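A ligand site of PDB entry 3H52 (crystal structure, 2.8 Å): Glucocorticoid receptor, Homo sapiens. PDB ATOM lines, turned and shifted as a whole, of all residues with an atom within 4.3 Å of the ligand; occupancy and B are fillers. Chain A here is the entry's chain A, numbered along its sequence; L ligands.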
ATOM      1  N   MET A  37      -9.530 -14.491 -15.861  1.00  0.00           N
ATOM      2  CA  MET A  37      -9.712 -15.663 -14.998  1.00  0.00           C
ATOM      3  C   MET A  37     -10.599 -15.361 -13.809  1.00  0.00           C
ATOM      4  O   MET A  37     -11.262 -16.250 -13.288  1.00  0.00           O
ATOM      5  CB  MET A  37      -8.369 -16.244 -14.542  1.00  0.00           C
ATOM      6  CG  MET A  37      -7.611 -17.058 -15.620  1.00  0.00           C
ATOM      7  SD  MET A  37      -8.524 -18.486 -16.272  1.00  0.00           S
ATOM      8  CE  MET A  37      -8.761 -19.518 -14.798  1.00  0.00           C
ATOM      9  N   LEU A  40     -14.231 -15.270 -15.414  1.00  0.00           N
ATOM     10  CA  LEU A  40     -14.755 -16.599 -15.702  1.00  0.00           C
ATOM     11  C   LEU A  40     -15.240 -17.279 -14.439  1.00  0.00           C
ATOM     12  O   LEU A  40     -16.343 -17.815 -14.397  1.00  0.00           O
ATOM     13  CB  LEU A  40     -13.692 -17.467 -16.403  1.00  0.00           C
ATOM     14  CG  LEU A  40     -13.529 -17.128 -17.879  1.00  0.00           C
ATOM     15  CD1 LEU A  40     -12.304 -17.847 -18.446  1.00  0.00           C
ATOM     16  CD2 LEU A  40     -14.809 -17.467 -18.646  1.00  0.00           C
ATOM     17  N   ASN A  41     -14.399 -17.228 -13.409  1.00  0.00           N
ATOM     18  CA  ASN A  41     -14.711 -17.833 -12.113  1.00  0.00           C
ATOM     19  C   ASN A  41     -16.067 -17.369 -11.561  1.00  0.00           C
ATOM     20  O   ASN A  41     -16.903 -18.197 -11.181  1.00  0.00           O
ATOM     21  CB  ASN A  41     -13.581 -17.578 -11.114  1.00  0.00           C
ATOM     22  CG  ASN A  41     -12.277 -18.319 -11.492  1.00  0.00           C
ATOM     23  OD1 ASN A  41     -12.234 -19.046 -12.500  1.00  0.00           O
ATOM     24  ND2 ASN A  41     -11.222 -18.113 -10.702  1.00  0.00           N
ATOM     25  N   GLY A  44     -18.625 -18.682 -14.013  1.00  0.00           N
ATOM     26  CA  GLY A  44     -18.747 -20.100 -13.667  1.00  0.00           C
ATOM     27  C   GLY A  44     -19.702 -20.302 -12.518  1.00  0.00           C
ATOM     28  O   GLY A  44     -20.666 -21.039 -12.633  1.00  0.00           O
ATOM     29  N   GLY A  45     -19.454 -19.617 -11.395  1.00  0.00           N
ATOM     30  CA  GLY A  45     -20.361 -19.645 -10.246  1.00  0.00           C
ATOM     31  C   GLY A  45     -21.809 -19.425 -10.623  1.00  0.00           C
ATOM     32  O   GLY A  45     -22.692 -20.174 -10.216  1.00  0.00           O
ATOM     33  N   GLN A  47     -23.128 -19.850 -13.554  1.00  0.00           N
ATOM     34  CA  GLN A  47     -23.600 -20.893 -14.439  1.00  0.00           C
ATOM     35  C   GLN A  47     -24.009 -22.160 -13.690  1.00  0.00           C
ATOM     36  O   GLN A  47     -24.910 -22.885 -14.120  1.00  0.00           O
ATOM     37  CB  GLN A  47     -22.528 -21.206 -15.484  1.00  0.00           C
ATOM     38  CG  GLN A  47     -22.559 -20.266 -16.679  1.00  0.00           C
ATOM     39  CD  GLN A  47     -21.532 -20.639 -17.747  1.00  0.00           C
ATOM     40  OE1 GLN A  47     -21.328 -19.907 -18.716  1.00  0.00           O
ATOM     41  NE2 GLN A  47     -20.880 -21.796 -17.562  1.00  0.00           N
ATOM     42  N   VAL A  48     -23.336 -22.422 -12.567  1.00  0.00           N
ATOM     43  CA  VAL A  48     -23.665 -23.542 -11.684  1.00  0.00           C
ATOM     44  C   VAL A  48     -25.049 -23.305 -11.087  1.00  0.00           C
ATOM     45  O   VAL A  48     -25.928 -24.183 -11.099  1.00  0.00           O
ATOM     46  CB  VAL A  48     -22.622 -23.695 -10.568  1.00  0.00           C
ATOM     47  CG1 VAL A  48     -22.998 -24.828  -9.605  1.00  0.00           C
ATOM     48  CG2 VAL A  48     -21.228 -23.958 -11.161  1.00  0.00           C
ATOM     49  N   TRP A  77     -21.840 -31.127 -13.012  1.00  0.00           N
ATOM     50  CA  TRP A  77     -21.948 -29.701 -13.307  1.00  0.00           C
ATOM     51  C   TRP A  77     -20.898 -29.251 -14.303  1.00  0.00           C
ATOM     52  O   TRP A  77     -21.213 -28.495 -15.217  1.00  0.00           O
ATOM     53  CB  TRP A  77     -21.927 -28.844 -12.036  1.00  0.00           C
ATOM     54  CG  TRP A  77     -20.688 -28.941 -11.241  1.00  0.00           C
ATOM     55  CD1 TRP A  77     -20.474 -29.734 -10.161  1.00  0.00           C
ATOM     56  CD2 TRP A  77     -19.476 -28.188 -11.442  1.00  0.00           C
ATOM     57  NE1 TRP A  77     -19.198 -29.536  -9.680  1.00  0.00           N
ATOM     58  CE2 TRP A  77     -18.570 -28.595 -10.456  1.00  0.00           C
ATOM     59  CE3 TRP A  77     -19.077 -27.233 -12.371  1.00  0.00           C
ATOM     60  CZ2 TRP A  77     -17.295 -28.078 -10.373  1.00  0.00           C
ATOM     61  CZ3 TRP A  77     -17.794 -26.718 -12.278  1.00  0.00           C
ATOM     62  CH2 TRP A  77     -16.932 -27.134 -11.286  1.00  0.00           C
ATOM     63  N   MET A  78     -19.676 -29.737 -14.143  1.00  0.00           N
ATOM     64  CA  MET A  78     -18.594 -29.397 -15.087  1.00  0.00           C
ATOM     65  C   MET A  78     -18.844 -29.977 -16.463  1.00  0.00           C
ATOM     66  O   MET A  78     -18.737 -29.266 -17.460  1.00  0.00           O
ATOM     67  CB  MET A  78     -17.244 -29.905 -14.584  1.00  0.00           C
ATOM     68  CG  MET A  78     -16.068 -29.562 -15.502  1.00  0.00           C
ATOM     69  SD  MET A  78     -15.794 -27.788 -15.697  1.00  0.00           S
ATOM     70  CE  MET A  78     -14.604 -27.518 -14.375  1.00  0.00           C
ATOM     71  N   MET A  81     -21.705 -27.818 -17.961  1.00  0.00           N
ATOM     72  CA  MET A  81     -21.248 -26.495 -18.339  1.00  0.00           C
ATOM     73  C   MET A  81     -20.287 -26.547 -19.505  1.00  0.00           C
ATOM     74  O   MET A  81     -20.426 -25.744 -20.421  1.00  0.00           O
ATOM     75  CB  MET A  81     -20.600 -25.794 -17.157  1.00  0.00           C
ATOM     76  CG  MET A  81     -21.560 -24.963 -16.373  1.00  0.00           C
ATOM     77  SD  MET A  81     -20.782 -24.348 -14.899  1.00  0.00           S
ATOM     78  CE  MET A  81     -21.541 -25.428 -13.717  1.00  0.00           C
ATOM     79  N   ALA A  82     -19.334 -27.485 -19.467  1.00  0.00           N
ATOM     80  CA  ALA A  82     -18.360 -27.651 -20.558  1.00  0.00           C
ATOM     81  C   ALA A  82     -19.031 -27.967 -21.876  1.00  0.00           C
ATOM     82  O   ALA A  82     -18.631 -27.478 -22.919  1.00  0.00           O
ATOM     83  CB  ALA A  82     -17.358 -28.752 -20.229  1.00  0.00           C
ATOM     84  N   LEU A  85     -20.771 -24.876 -23.204  1.00  0.00           N
ATOM     85  CA  LEU A  85     -19.725 -24.009 -23.763  1.00  0.00           C
ATOM     86  C   LEU A  85     -19.316 -24.503 -25.143  1.00  0.00           C
ATOM     87  O   LEU A  85     -19.097 -23.709 -26.047  1.00  0.00           O
ATOM     88  CB  LEU A  85     -18.489 -23.965 -22.850  1.00  0.00           C
ATOM     89  CG  LEU A  85     -17.283 -23.167 -23.378  1.00  0.00           C
ATOM     90  CD1 LEU A  85     -17.609 -21.688 -23.431  1.00  0.00           C
ATOM     91  CD2 LEU A  85     -16.050 -23.413 -22.537  1.00  0.00           C
ATOM     92  N   ARG A  88     -22.562 -23.375 -27.336  1.00  0.00           N
ATOM     93  CA  ARG A  88     -22.482 -21.922 -27.547  1.00  0.00           C
ATOM     94  C   ARG A  88     -21.394 -21.567 -28.558  1.00  0.00           C
ATOM     95  O   ARG A  88     -21.630 -20.786 -29.465  1.00  0.00           O
ATOM     96  CB  ARG A  88     -22.231 -21.173 -26.227  1.00  0.00           C
ATOM     97  CG  ARG A  88     -23.497 -20.814 -25.504  1.00  0.00           C
ATOM     98  CD  ARG A  88     -23.292 -19.763 -24.439  1.00  0.00           C
ATOM     99  NE  ARG A  88     -22.252 -20.079 -23.458  1.00  0.00           N
ATOM    100  CZ  ARG A  88     -22.266 -21.117 -22.618  1.00  0.00           C
ATOM    101  NH1 ARG A  88     -23.251 -22.009 -22.640  1.00  0.00           N
ATOM    102  NH2 ARG A  88     -21.268 -21.270 -21.760  1.00  0.00           N
ATOM    103  N   PHE A 100     -17.468 -18.179 -24.276  1.00  0.00           N
ATOM    104  CA  PHE A 100     -17.790 -18.235 -22.848  1.00  0.00           C
ATOM    105  C   PHE A 100     -19.088 -17.492 -22.520  1.00  0.00           C
ATOM    106  O   PHE A 100     -19.902 -17.966 -21.730  1.00  0.00           O
ATOM    107  CB  PHE A 100     -16.628 -17.687 -22.023  1.00  0.00           C
ATOM    108  CG  PHE A 100     -15.493 -18.657 -21.872  1.00  0.00           C
ATOM    109  CD1 PHE A 100     -14.243 -18.364 -22.391  1.00  0.00           C
ATOM    110  CD2 PHE A 100     -15.683 -19.867 -21.223  1.00  0.00           C
ATOM    111  CE1 PHE A 100     -13.201 -19.272 -22.253  1.00  0.00           C
ATOM    112  CE2 PHE A 100     -14.655 -20.773 -21.083  1.00  0.00           C
ATOM    113  CZ  PHE A 100     -13.410 -20.480 -21.589  1.00  0.00           C
ATOM    114  N   MET A 116      -3.981 -19.869 -21.138  1.00  0.00           N
ATOM    115  CA  MET A 116      -5.189 -20.471 -21.708  1.00  0.00           C
ATOM    116  C   MET A 116      -4.986 -21.870 -22.276  1.00  0.00           C
ATOM    117  O   MET A 116      -5.906 -22.691 -22.215  1.00  0.00           O
ATOM    118  CB  MET A 116      -5.719 -19.605 -22.840  1.00  0.00           C
ATOM    119  CG  MET A 116      -6.176 -18.236 -22.397  1.00  0.00           C
ATOM    120  SD  MET A 116      -7.621 -18.344 -21.356  1.00  0.00           S
ATOM    121  CE  MET A 116      -6.869 -18.422 -19.731  1.00  0.00           C
ATOM    122  N   GLN A 119      -6.054 -25.642 -21.010  1.00  0.00           N
ATOM    123  CA  GLN A 119      -7.497 -25.780 -20.762  1.00  0.00           C
ATOM    124  C   GLN A 119      -8.321 -25.749 -22.036  1.00  0.00           C
ATOM    125  O   GLN A 119      -9.186 -26.594 -22.255  1.00  0.00           O
ATOM    126  CB  GLN A 119      -8.036 -24.658 -19.847  1.00  0.00           C
ATOM    127  CG  GLN A 119      -7.116 -24.172 -18.757  1.00  0.00           C
ATOM    128  CD  GLN A 119      -6.501 -22.824 -19.091  1.00  0.00           C
ATOM    129  OE1 GLN A 119      -7.147 -21.788 -18.947  1.00  0.00           O
ATOM    130  NE2 GLN A 119      -5.243 -22.839 -19.527  1.00  0.00           N
ATOM    131  N   MET A 123     -11.743 -27.642 -24.031  1.00  0.00           N
ATOM    132  CA  MET A 123     -13.054 -27.040 -24.249  1.00  0.00           C
ATOM    133  C   MET A 123     -13.366 -26.917 -25.741  1.00  0.00           C
ATOM    134  O   MET A 123     -14.494 -27.154 -26.166  1.00  0.00           O
ATOM    135  CB  MET A 123     -13.171 -25.686 -23.513  1.00  0.00           C
ATOM    136  CG  MET A 123     -13.408 -25.865 -22.006  1.00  0.00           C
ATOM    137  SD  MET A 123     -13.068 -24.424 -21.010  1.00  0.00           S
ATOM    138  CE  MET A 123     -11.291 -24.511 -20.905  1.00  0.00           C
ATOM    139  N   LEU A 209      -9.873 -31.564 -17.479  1.00  0.00           N
ATOM    140  CA  LEU A 209     -10.094 -30.226 -16.909  1.00  0.00           C
ATOM    141  C   LEU A 209      -9.836 -30.221 -15.402  1.00  0.00           C
ATOM    142  O   LEU A 209      -9.224 -29.297 -14.878  1.00  0.00           O
ATOM    143  CB  LEU A 209     -11.510 -29.723 -17.196  1.00  0.00           C
ATOM    144  CG  LEU A 209     -11.755 -29.124 -18.579  1.00  0.00           C
ATOM    145  CD1 LEU A 209     -13.252 -28.849 -18.832  1.00  0.00           C
ATOM    146  CD2 LEU A 209     -10.939 -27.862 -18.754  1.00  0.00           C
ATOM    147  N   TYR A 212      -6.128 -30.645 -14.790  1.00  0.00           N
ATOM    148  CA  TYR A 212      -5.506 -29.336 -15.000  1.00  0.00           C
ATOM    149  C   TYR A 212      -5.604 -28.502 -13.721  1.00  0.00           C
ATOM    150  O   TYR A 212      -4.619 -27.913 -13.287  1.00  0.00           O
ATOM    151  CB  TYR A 212      -6.145 -28.576 -16.178  1.00  0.00           C
ATOM    152  CG  TYR A 212      -6.043 -27.063 -16.080  1.00  0.00           C
ATOM    153  CD1 TYR A 212      -7.102 -26.302 -15.573  1.00  0.00           C
ATOM    154  CD2 TYR A 212      -4.883 -26.393 -16.479  1.00  0.00           C
ATOM    155  CE1 TYR A 212      -7.015 -24.916 -15.463  1.00  0.00           C
ATOM    156  CE2 TYR A 212      -4.787 -24.997 -16.374  1.00  0.00           C
ATOM    157  CZ  TYR A 212      -5.867 -24.267 -15.867  1.00  0.00           C
ATOM    158  OH  TYR A 212      -5.792 -22.896 -15.769  1.00  0.00           O
ATOM    159  N   MET A 229     -11.068 -20.835  -5.412  1.00  0.00           N
ATOM    160  CA  MET A 229     -11.905 -21.169  -6.572  1.00  0.00           C
ATOM    161  C   MET A 229     -11.424 -22.466  -7.203  1.00  0.00           C
ATOM    162  O   MET A 229     -12.235 -23.369  -7.432  1.00  0.00           O
ATOM    163  CB  MET A 229     -11.899 -20.034  -7.605  1.00  0.00           C
ATOM    164  CG  MET A 229     -12.564 -18.723  -7.155  1.00  0.00           C
ATOM    165  SD  MET A 229     -14.338 -18.603  -7.532  1.00  0.00           S
ATOM    166  CE  MET A 229     -15.044 -19.831  -6.434  1.00  0.00           C
ATOM    167  N   LEU A 230     -10.117 -22.578  -7.461  1.00  0.00           N
ATOM    168  CA  LEU A 230      -9.521 -23.822  -7.998  1.00  0.00           C
ATOM    169  C   LEU A 230      -9.382 -24.917  -6.934  1.00  0.00           C
ATOM    170  O   LEU A 230      -9.046 -26.056  -7.274  1.00  0.00           O
ATOM    171  CB  LEU A 230      -8.145 -23.543  -8.621  1.00  0.00           C
ATOM    172  CG  LEU A 230      -8.034 -22.523  -9.765  1.00  0.00           C
ATOM    173  CD1 LEU A 230      -6.571 -22.188 -10.032  1.00  0.00           C
ATOM    174  CD2 LEU A 230      -8.710 -23.012 -11.044  1.00  0.00           C
ATOM    175  N   ILE A 233     -13.240 -26.287  -6.367  1.00  0.00           N
ATOM    176  CA  ILE A 233     -13.465 -27.200  -7.486  1.00  0.00           C
ATOM    177  C   ILE A 233     -12.940 -28.628  -7.186  1.00  0.00           C
ATOM    178  O   ILE A 233     -13.399 -29.597  -7.788  1.00  0.00           O
ATOM    179  CB  ILE A 233     -12.863 -26.646  -8.817  1.00  0.00           C
ATOM    180  CG1 ILE A 233     -13.712 -25.497  -9.370  1.00  0.00           C
ATOM    181  CG2 ILE A 233     -12.796 -27.727  -9.886  1.00  0.00           C
ATOM    182  CD1 ILE A 233     -13.212 -24.952 -10.694  1.00  0.00           C
HETATM  183  O1  LIG L   1     -19.140 -21.024 -19.642  1.00  0.00           O
HETATM  184  C1  LIG L   1     -18.324 -21.409 -18.819  1.00  0.00           C
HETATM  185  C2  LIG L   1     -17.650 -20.364 -17.949  1.00  0.00           C
HETATM  186  C3  LIG L   1     -18.016 -22.776 -18.699  1.00  0.00           C
HETATM  187  C4  LIG L   1     -17.099 -23.227 -17.814  1.00  0.00           C
HETATM  188  C5  LIG L   1     -16.754 -24.691 -17.671  1.00  0.00           C
HETATM  189  C6  LIG L   1     -16.401 -22.300 -16.926  1.00  0.00           C
HETATM  190  C7  LIG L   1     -17.034 -20.948 -16.677  1.00  0.00           C
HETATM  191  C8  LIG L   1     -15.247 -22.644 -16.347  1.00  0.00           C
HETATM  192  C9  LIG L   1     -14.592 -21.634 -15.416  1.00  0.00           C
HETATM  193  C10 LIG L   1     -15.182 -21.829 -14.033  1.00  0.00           C
HETATM  194  C11 LIG L   1     -14.517 -21.376 -12.901  1.00  0.00           C
HETATM  195  C12 LIG L   1     -15.043 -21.547 -11.630  1.00  0.00           C
HETATM  196  C13 LIG L   1     -16.264 -22.177 -11.495  1.00  0.00           C
HETATM  197  N1  LIG L   1     -16.812 -22.349 -10.225  1.00  0.00           N
HETATM  198  C14 LIG L   1     -16.078 -21.859  -9.076  1.00  0.00           C
HETATM  199  C15 LIG L   1     -18.107 -23.030 -10.079  1.00  0.00           C
HETATM  200  C16 LIG L   1     -16.929 -22.629 -12.627  1.00  0.00           C
HETATM  201  C17 LIG L   1     -16.408 -22.458 -13.885  1.00  0.00           C
HETATM  202  C18 LIG L   1     -13.047 -21.720 -15.344  1.00  0.00           C
HETATM  203  C19 LIG L   1     -12.515 -23.131 -15.525  1.00  0.00           C
HETATM  204  C20 LIG L   1     -12.834 -24.008 -14.310  1.00  0.00           C
HETATM  205  C21 LIG L   1     -11.023 -23.274 -15.902  1.00  0.00           C
HETATM  206  C22 LIG L   1     -10.703 -22.384 -17.042  1.00  0.00           C
HETATM  207  C23 LIG L   1     -10.496 -21.675 -17.963  1.00  0.00           C
HETATM  208  C24 LIG L   1     -10.181 -20.875 -19.164  1.00  0.00           C
HETATM  209  O2  LIG L   1     -10.115 -23.026 -14.828  1.00  0.00           O
HETATM  210  C25 LIG L   1     -10.928 -24.754 -16.328  1.00  0.00           C
HETATM  211  C26 LIG L   1     -12.332 -25.080 -16.900  1.00  0.00           C
HETATM  212  C27 LIG L   1     -13.129 -23.763 -16.794  1.00  0.00           C
HETATM  213  C28 LIG L   1     -14.612 -23.980 -16.558  1.00  0.00           C
HETATM  214  C29 LIG L   1     -15.225 -24.755 -17.711  1.00  0.00           C
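The guanidinium group (NH2) of Arg 88 lies within hydrogen-bond range of an oxygen (O1) of the ligand. The side-chain amide oxygen (OE1) of Gln 47 lies close to an oxygen (O1) of the ligand, 2.6 Å away.
SD of Met 81 lies close to NE2 of Gln 47 (3.7 Å). NE2 of Gln 119 sits at hydrogen-bond distance from O of Met 116 (2.8 Å). The side-chain amide oxygen of Gln 47 is in hydrogen-bond range of the guanidinium group of Arg 88 (3.3 Å). The backbone carbonyl oxygen (O) of Met 37 lies close to the side-chain amide oxygen (OD1) of Asn 41 (3.1 Å).
Met 37 touches the ligand (CE to O2, 3.8 Å). Leu 40 touches the ligand. Asn 41 touches the ligand (OD1 to C11, 3.3 Å). Gly 44 touches the ligand (CA to C16, 3.3 Å). N of Gly 45 touches C15 of the ligand, 3.9 Å away. Val 48 touches the ligand. Met 78 touches the ligand. Phe 100 touches the ligand. OE1 of Gln 119 touches C24 of the ligand, 3.2 Å away. Met 123 touches the ligand (SD to C29, 3.96 Å). Leu 209 touches the ligand (CD2 to C26, 3.6 Å). CE1 of Tyr 212 touches O2 of the ligand, at 3.7 Å. CE of Met 229 touches C14 of the ligand, at 3.5 Å. CD1 of Ile 233 touches C20 of the ligand, 3.8 Å away. Within 4 Å of the ligand: Met 37, Leu 40, Asn 41, Gly 44, Gly 45, Gln 47, Val 48, Met 78, Arg 88, Phe 100, Gln 119, Met 123, Leu 209, Tyr 212, Met 229 and Ile 233. The nearest printed residue that does not touch the ligand is Met 81 (4.03 Å).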
